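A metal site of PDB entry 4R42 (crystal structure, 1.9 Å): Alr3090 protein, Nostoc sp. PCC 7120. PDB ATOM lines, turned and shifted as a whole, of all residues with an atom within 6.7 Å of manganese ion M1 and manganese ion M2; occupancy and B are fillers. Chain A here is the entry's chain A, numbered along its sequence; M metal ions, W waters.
Of the 22 residues printed, 4 come within 4 Å of manganese ion M1. Along chain A the residues within 4 Å of manganese ion M1 span positions 35 to 163.
Of the 22 residues printed, 4 come within 4 Å of manganese ion M2. Along chain A the residues within 4 Å of manganese ion M2 span positions 65 to 166.
The side-chain hydroxyl (OG1) of Thr 167 lies within hydrogen-bond range of the backbone carbonyl oxygen (O) of Glu 163, 2.8 Å away. OE1 of Glu 35 sits close to OH of Tyr 140. O of Gln 28 lies within hydrogen-bond range of N of Glu 35, 2.9 Å away. OE2 of Glu 133 sits close to OH of Tyr 42, at 2.6 Å. A ring nitrogen (NE2) of His 68 is in hydrogen-bond range of the side-chain carboxylate (OE2) of Glu 64 (2.9 Å). ND1 of His 166 sits close to O of Arg 162 (3.4 Å). OE1 of Glu 64 lies within hydrogen-bond range of NE2 of His 166, at 2.8 Å.
Manganese ion M2 is bound by OE2 of Glu 65 (2.1 Å), OE1 of Glu 163 (2.1 Å), water W2 (2.2 Å), OE2 of Glu 133 (2.3 Å), ND1 of His 166 (2.3 Å) and OE1 of Glu 133 (2.3 Å).
Manganese ion M1 is bound by OE2 of Glu 163 (2.1 Å), OE1 of Glu 65 (2.1 Å), OE2 of Glu 35 (2.2 Å), ND1 of His 68 (2.3 Å), OE1 of Glu 35 (2.4 Å) and water W1 (2.5 Å). Manganese ion M1 has six donor atoms within binding distance.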
ATOM      1  N   GLN A  28      25.487   7.336  -8.363  1.00  0.00           N
ATOM      2  CA  GLN A  28      25.790   6.637  -9.612  1.00  0.00           C
ATOM      3  C   GLN A  28      25.842   5.120  -9.416  1.00  0.00           C
ATOM      4  O   GLN A  28      26.056   4.375 -10.379  1.00  0.00           O
ATOM      5  CB  GLN A  28      27.090   7.164 -10.232  1.00  0.00           C
ATOM      6  CG  GLN A  28      26.958   8.584 -10.807  1.00  0.00           C
ATOM      7  CD  GLN A  28      25.712   8.769 -11.664  1.00  0.00           C
ATOM      8  OE1 GLN A  28      24.654   9.180 -11.171  1.00  0.00           O
ATOM      9  NE2 GLN A  28      25.822   8.441 -12.939  1.00  0.00           N
ATOM     10  N   GLY A  34      21.987   6.727 -12.111  1.00  0.00           N
ATOM     11  CA  GLY A  34      23.124   5.839 -11.952  1.00  0.00           C
ATOM     12  C   GLY A  34      23.261   4.672 -12.902  1.00  0.00           C
ATOM     13  O   GLY A  34      22.473   4.494 -13.839  1.00  0.00           O
ATOM     14  N   GLU A  35      24.277   3.857 -12.628  1.00  0.00           N
ATOM     15  CA  GLU A  35      24.697   2.815 -13.524  1.00  0.00           C
ATOM     16  C   GLU A  35      23.738   1.628 -13.523  1.00  0.00           C
ATOM     17  O   GLU A  35      23.603   0.965 -14.547  1.00  0.00           O
ATOM     18  CB  GLU A  35      26.102   2.340 -13.167  1.00  0.00           C
ATOM     19  CG  GLU A  35      27.163   3.420 -13.302  1.00  0.00           C
ATOM     20  CD  GLU A  35      27.357   3.892 -14.729  1.00  0.00           C
ATOM     21  OE1 GLU A  35      28.034   4.922 -14.946  1.00  0.00           O
ATOM     22  OE2 GLU A  35      26.852   3.215 -15.659  1.00  0.00           O
ATOM     23  N   ALA A  38      20.931   2.650 -15.863  1.00  0.00           N
ATOM     24  CA  ALA A  38      21.306   2.568 -17.257  1.00  0.00           C
ATOM     25  C   ALA A  38      21.326   1.104 -17.710  1.00  0.00           C
ATOM     26  O   ALA A  38      20.694   0.757 -18.715  1.00  0.00           O
ATOM     27  CB  ALA A  38      22.669   3.235 -17.503  1.00  0.00           C
ATOM     28  N   TYR A  42      18.450  -0.388 -20.469  1.00  0.00           N
ATOM     29  CA  TYR A  42      18.817  -0.813 -21.814  1.00  0.00           C
ATOM     30  C   TYR A  42      18.620  -2.316 -21.949  1.00  0.00           C
ATOM     31  O   TYR A  42      18.180  -2.794 -22.988  1.00  0.00           O
ATOM     32  CB  TYR A  42      20.261  -0.419 -22.144  1.00  0.00           C
ATOM     33  CG  TYR A  42      20.591   1.029 -21.851  1.00  0.00           C
ATOM     34  CD1 TYR A  42      19.585   2.000 -21.825  1.00  0.00           C
ATOM     35  CD2 TYR A  42      21.890   1.435 -21.592  1.00  0.00           C
ATOM     36  CE1 TYR A  42      19.887   3.316 -21.520  1.00  0.00           C
ATOM     37  CE2 TYR A  42      22.194   2.743 -21.282  1.00  0.00           C
ATOM     38  CZ  TYR A  42      21.182   3.680 -21.247  1.00  0.00           C
ATOM     39  OH  TYR A  42      21.461   4.995 -20.950  1.00  0.00           O
ATOM     40  N   ILE A  61      25.803  -1.890 -24.814  1.00  0.00           N
ATOM     41  CA  ILE A  61      25.903  -0.757 -23.893  1.00  0.00           C
ATOM     42  C   ILE A  61      25.492  -1.167 -22.459  1.00  0.00           C
ATOM     43  O   ILE A  61      26.177  -0.805 -21.510  1.00  0.00           O
ATOM     44  CB  ILE A  61      25.037   0.437 -24.370  1.00  0.00           C
ATOM     45  CG1 ILE A  61      25.540   0.914 -25.740  1.00  0.00           C
ATOM     46  CG2 ILE A  61      25.089   1.566 -23.348  1.00  0.00           C
ATOM     47  CD1 ILE A  61      24.664   2.001 -26.403  1.00  0.00           C
ATOM     48  N   GLU A  64      28.363  -2.716 -20.749  1.00  0.00           N
ATOM     49  CA  GLU A  64      29.335  -1.703 -20.321  1.00  0.00           C
ATOM     50  C   GLU A  64      28.860  -0.978 -19.065  1.00  0.00           C
ATOM     51  O   GLU A  64      29.665  -0.664 -18.196  1.00  0.00           O
ATOM     52  CB  GLU A  64      29.621  -0.665 -21.408  1.00  0.00           C
ATOM     53  CG  GLU A  64      30.805   0.196 -20.999  1.00  0.00           C
ATOM     54  CD  GLU A  64      31.180   1.294 -21.964  1.00  0.00           C
ATOM     55  OE1 GLU A  64      30.636   1.347 -23.081  1.00  0.00           O
ATOM     56  OE2 GLU A  64      32.052   2.107 -21.597  1.00  0.00           O
ATOM     57  N   GLU A  65      27.558  -0.675 -18.977  1.00  0.00           N
ATOM     58  CA  GLU A  65      27.047   0.016 -17.801  1.00  0.00           C
ATOM     59  C   GLU A  65      27.227  -0.831 -16.534  1.00  0.00           C
ATOM     60  O   GLU A  65      27.516  -0.301 -15.462  1.00  0.00           O
ATOM     61  CB  GLU A  65      25.561   0.394 -17.976  1.00  0.00           C
ATOM     62  CG  GLU A  65      25.249   1.225 -19.221  1.00  0.00           C
ATOM     63  CD  GLU A  65      25.775   2.671 -19.205  1.00  0.00           C
ATOM     64  OE1 GLU A  65      26.792   2.963 -18.544  1.00  0.00           O
ATOM     65  OE2 GLU A  65      25.173   3.520 -19.891  1.00  0.00           O
ATOM     66  N   PHE A  66      27.085  -2.142 -16.665  1.00  0.00           N
ATOM     67  CA  PHE A  66      27.355  -3.040 -15.538  1.00  0.00           C
ATOM     68  C   PHE A  66      28.818  -2.954 -15.140  1.00  0.00           C
ATOM     69  O   PHE A  66      29.160  -3.041 -13.960  1.00  0.00           O
ATOM     70  CB  PHE A  66      27.003  -4.493 -15.880  1.00  0.00           C
ATOM     71  CG  PHE A  66      25.536  -4.846 -15.724  1.00  0.00           C
ATOM     72  CD1 PHE A  66      24.858  -4.571 -14.539  1.00  0.00           C
ATOM     73  CD2 PHE A  66      24.852  -5.455 -16.758  1.00  0.00           C
ATOM     74  CE1 PHE A  66      23.506  -4.925 -14.400  1.00  0.00           C
ATOM     75  CE2 PHE A  66      23.504  -5.796 -16.621  1.00  0.00           C
ATOM     76  CZ  PHE A  66      22.842  -5.534 -15.444  1.00  0.00           C
ATOM     77  N   HIS A  68      30.612  -0.240 -15.530  1.00  0.00           N
ATOM     78  CA  HIS A  68      30.682   1.048 -14.853  1.00  0.00           C
ATOM     79  C   HIS A  68      30.181   0.929 -13.410  1.00  0.00           C
ATOM     80  O   HIS A  68      30.748   1.519 -12.485  1.00  0.00           O
ATOM     81  CB  HIS A  68      29.833   2.115 -15.554  1.00  0.00           C
ATOM     82  CG  HIS A  68      30.304   2.497 -16.931  1.00  0.00           C
ATOM     83  ND1 HIS A  68      29.654   3.443 -17.691  1.00  0.00           N
ATOM     84  CD2 HIS A  68      31.359   2.075 -17.676  1.00  0.00           C
ATOM     85  CE1 HIS A  68      30.274   3.569 -18.855  1.00  0.00           C
ATOM     86  NE2 HIS A  68      31.313   2.760 -18.872  1.00  0.00           N
ATOM     87  N   LEU A  69      29.099   0.175 -13.215  1.00  0.00           N
ATOM     88  CA  LEU A  69      28.524  -0.030 -11.884  1.00  0.00           C
ATOM     89  C   LEU A  69      29.572  -0.652 -10.965  1.00  0.00           C
ATOM     90  O   LEU A  69      29.697  -0.277  -9.800  1.00  0.00           O
ATOM     91  CB  LEU A  69      27.284  -0.920 -11.967  1.00  0.00           C
ATOM     92  CG  LEU A  69      26.548  -1.210 -10.658  1.00  0.00           C
ATOM     93  CD1 LEU A  69      25.931   0.050 -10.054  1.00  0.00           C
ATOM     94  CD2 LEU A  69      25.493  -2.253 -10.919  1.00  0.00           C
ATOM     95  N   ALA A 132      18.432   9.420 -20.224  1.00  0.00           N
ATOM     96  CA  ALA A 132      19.091   8.740 -19.124  1.00  0.00           C
ATOM     97  C   ALA A 132      20.560   9.130 -19.131  1.00  0.00           C
ATOM     98  O   ALA A 132      21.111   9.506 -18.085  1.00  0.00           O
ATOM     99  CB  ALA A 132      18.929   7.219 -19.246  1.00  0.00           C
ATOM    100  N   GLU A 133      21.183   9.052 -20.307  1.00  0.00           N
ATOM    101  CA  GLU A 133      22.578   9.427 -20.471  1.00  0.00           C
ATOM    102  C   GLU A 133      22.806  10.877 -20.045  1.00  0.00           C
ATOM    103  O   GLU A 133      23.869  11.213 -19.534  1.00  0.00           O
ATOM    104  CB  GLU A 133      23.049   9.235 -21.915  1.00  0.00           C
ATOM    105  CG  GLU A 133      23.051   7.787 -22.406  1.00  0.00           C
ATOM    106  CD  GLU A 133      24.094   6.933 -21.719  1.00  0.00           C
ATOM    107  OE1 GLU A 133      25.145   7.468 -21.335  1.00  0.00           O
ATOM    108  OE2 GLU A 133      23.856   5.703 -21.582  1.00  0.00           O
ATOM    109  N   ALA A 136      22.886  10.952 -16.310  1.00  0.00           N
ATOM    110  CA  ALA A 136      24.127  10.323 -15.860  1.00  0.00           C
ATOM    111  C   ALA A 136      25.321  11.268 -16.025  1.00  0.00           C
ATOM    112  O   ALA A 136      26.129  11.438 -15.107  1.00  0.00           O
ATOM    113  CB  ALA A 136      24.373   9.009 -16.607  1.00  0.00           C
ATOM    114  N   TYR A 140      27.636  12.980 -13.020  1.00  0.00           N
ATOM    115  CA  TYR A 140      29.093  12.816 -13.011  1.00  0.00           C
ATOM    116  C   TYR A 140      29.756  14.184 -12.970  1.00  0.00           C
ATOM    117  O   TYR A 140      30.732  14.347 -12.237  1.00  0.00           O
ATOM    118  CB  TYR A 140      29.587  12.000 -14.224  1.00  0.00           C
ATOM    119  CG  TYR A 140      29.518  10.496 -13.993  1.00  0.00           C
ATOM    120  CD1 TYR A 140      30.106   9.930 -12.864  1.00  0.00           C
ATOM    121  CD2 TYR A 140      28.844   9.654 -14.875  1.00  0.00           C
ATOM    122  CE1 TYR A 140      30.032   8.562 -12.623  1.00  0.00           C
ATOM    123  CE2 TYR A 140      28.763   8.272 -14.649  1.00  0.00           C
ATOM    124  CZ  TYR A 140      29.352   7.736 -13.517  1.00  0.00           C
ATOM    125  OH  TYR A 140      29.285   6.391 -13.248  1.00  0.00           O
ATOM    126  N   LEU A 159      34.178   7.906 -16.911  1.00  0.00           N
ATOM    127  CA  LEU A 159      32.799   7.464 -16.910  1.00  0.00           C
ATOM    128  C   LEU A 159      31.915   8.499 -17.603  1.00  0.00           C
ATOM    129  O   LEU A 159      31.048   8.161 -18.390  1.00  0.00           O
ATOM    130  CB  LEU A 159      32.327   7.200 -15.480  1.00  0.00           C
ATOM    131  CG  LEU A 159      33.046   6.038 -14.795  1.00  0.00           C
ATOM    132  CD1 LEU A 159      32.799   6.046 -13.299  1.00  0.00           C
ATOM    133  CD2 LEU A 159      32.620   4.704 -15.425  1.00  0.00           C
ATOM    134  N   ARG A 162      32.370   8.217 -21.334  1.00  0.00           N
ATOM    135  CA  ARG A 162      31.622   7.083 -21.884  1.00  0.00           C
ATOM    136  C   ARG A 162      30.109   7.377 -22.020  1.00  0.00           C
ATOM    137  O   ARG A 162      29.467   6.822 -22.918  1.00  0.00           O
ATOM    138  CB  ARG A 162      31.847   5.827 -21.033  1.00  0.00           C
ATOM    139  CG  ARG A 162      33.316   5.332 -21.019  1.00  0.00           C
ATOM    140  CD  ARG A 162      33.866   5.096 -22.438  1.00  0.00           C
ATOM    141  NE  ARG A 162      32.981   4.195 -23.167  1.00  0.00           N
ATOM    142  CZ  ARG A 162      32.887   4.098 -24.493  1.00  0.00           C
ATOM    143  NH1 ARG A 162      33.625   4.860 -25.290  1.00  0.00           N
ATOM    144  NH2 ARG A 162      32.038   3.223 -25.018  1.00  0.00           N
ATOM    145  N   GLU A 163      29.529   8.233 -21.176  1.00  0.00           N
ATOM    146  CA  GLU A 163      28.123   8.550 -21.348  1.00  0.00           C
ATOM    147  C   GLU A 163      27.924   9.498 -22.559  1.00  0.00           C
ATOM    148  O   GLU A 163      26.876   9.462 -23.213  1.00  0.00           O
ATOM    149  CB  GLU A 163      27.494   9.175 -20.085  1.00  0.00           C
ATOM    150  CG  GLU A 163      27.794   8.512 -18.702  1.00  0.00           C
ATOM    151  CD  GLU A 163      27.738   6.965 -18.616  1.00  0.00           C
ATOM    152  OE1 GLU A 163      27.540   6.235 -19.615  1.00  0.00           O
ATOM    153  OE2 GLU A 163      27.926   6.477 -17.465  1.00  0.00           O
ATOM    154  N   ILE A 164      28.910  10.337 -22.873  1.00  0.00           N
ATOM    155  CA  ILE A 164      28.845  11.121 -24.102  1.00  0.00           C
ATOM    156  C   ILE A 164      28.894  10.151 -25.283  1.00  0.00           C
ATOM    157  O   ILE A 164      28.138  10.297 -26.238  1.00  0.00           O
ATOM    158  CB  ILE A 164      29.986  12.154 -24.164  1.00  0.00           C
ATOM    159  CG1 ILE A 164      29.764  13.213 -23.078  1.00  0.00           C
ATOM    160  CG2 ILE A 164      30.074  12.830 -25.533  1.00  0.00           C
ATOM    161  CD1 ILE A 164      30.981  14.034 -22.736  1.00  0.00           C
ATOM    162  N   HIS A 166      27.962   6.963 -25.365  1.00  0.00           N
ATOM    163  CA  HIS A 166      26.685   6.287 -25.442  1.00  0.00           C
ATOM    164  C   HIS A 166      25.621   7.189 -26.023  1.00  0.00           C
ATOM    165  O   HIS A 166      24.768   6.729 -26.788  1.00  0.00           O
ATOM    166  CB  HIS A 166      26.235   5.809 -24.063  1.00  0.00           C
ATOM    167  CG  HIS A 166      27.128   4.799 -23.460  1.00  0.00           C
ATOM    168  ND1 HIS A 166      27.080   4.465 -22.122  1.00  0.00           N
ATOM    169  CD2 HIS A 166      28.087   4.011 -24.010  1.00  0.00           C
ATOM    170  CE1 HIS A 166      27.979   3.528 -21.870  1.00  0.00           C
ATOM    171  NE2 HIS A 166      28.610   3.245 -22.995  1.00  0.00           N
ATOM    172  N   THR A 167      25.634   8.450 -25.629  1.00  0.00           N
ATOM    173  CA  THR A 167      24.665   9.407 -26.182  1.00  0.00           C
ATOM    174  C   THR A 167      24.771   9.419 -27.709  1.00  0.00           C
ATOM    175  O   THR A 167      23.775   9.405 -28.424  1.00  0.00           O
ATOM    176  CB  THR A 167      24.898  10.843 -25.656  1.00  0.00           C
ATOM    177  OG1 THR A 167      24.728  10.848 -24.231  1.00  0.00           O
ATOM    178  CG2 THR A 167      23.902  11.830 -26.294  1.00  0.00           C
ATOM    179  N   PHE A 170      23.222   6.212 -29.174  1.00  0.00           N
ATOM    180  CA  PHE A 170      21.761   6.327 -29.226  1.00  0.00           C
ATOM    181  C   PHE A 170      21.277   7.331 -30.273  1.00  0.00           C
ATOM    182  O   PHE A 170      20.243   7.127 -30.931  1.00  0.00           O
ATOM    183  CB  PHE A 170      21.221   6.708 -27.829  1.00  0.00           C
ATOM    184  CG  PHE A 170      21.388   5.615 -26.810  1.00  0.00           C
ATOM    185  CD1 PHE A 170      20.922   4.336 -27.044  1.00  0.00           C
ATOM    186  CD2 PHE A 170      22.029   5.868 -25.607  1.00  0.00           C
ATOM    187  CE1 PHE A 170      21.079   3.335 -26.104  1.00  0.00           C
ATOM    188  CE2 PHE A 170      22.195   4.857 -24.668  1.00  0.00           C
ATOM    189  CZ  PHE A 170      21.721   3.601 -24.921  1.00  0.00           C
HETATM  190 MN    MN M   1      27.661   4.449 -17.267  1.00  0.00          MN
HETATM  191 MN    MN M   2      25.806   5.413 -20.461  1.00  0.00          MN
HETATM  192  O   HOH W   1      25.358   5.292 -16.714  1.00  0.00           O
HETATM  193  O   HOH W   2      24.779   6.228 -18.672  1.00  0.00           O
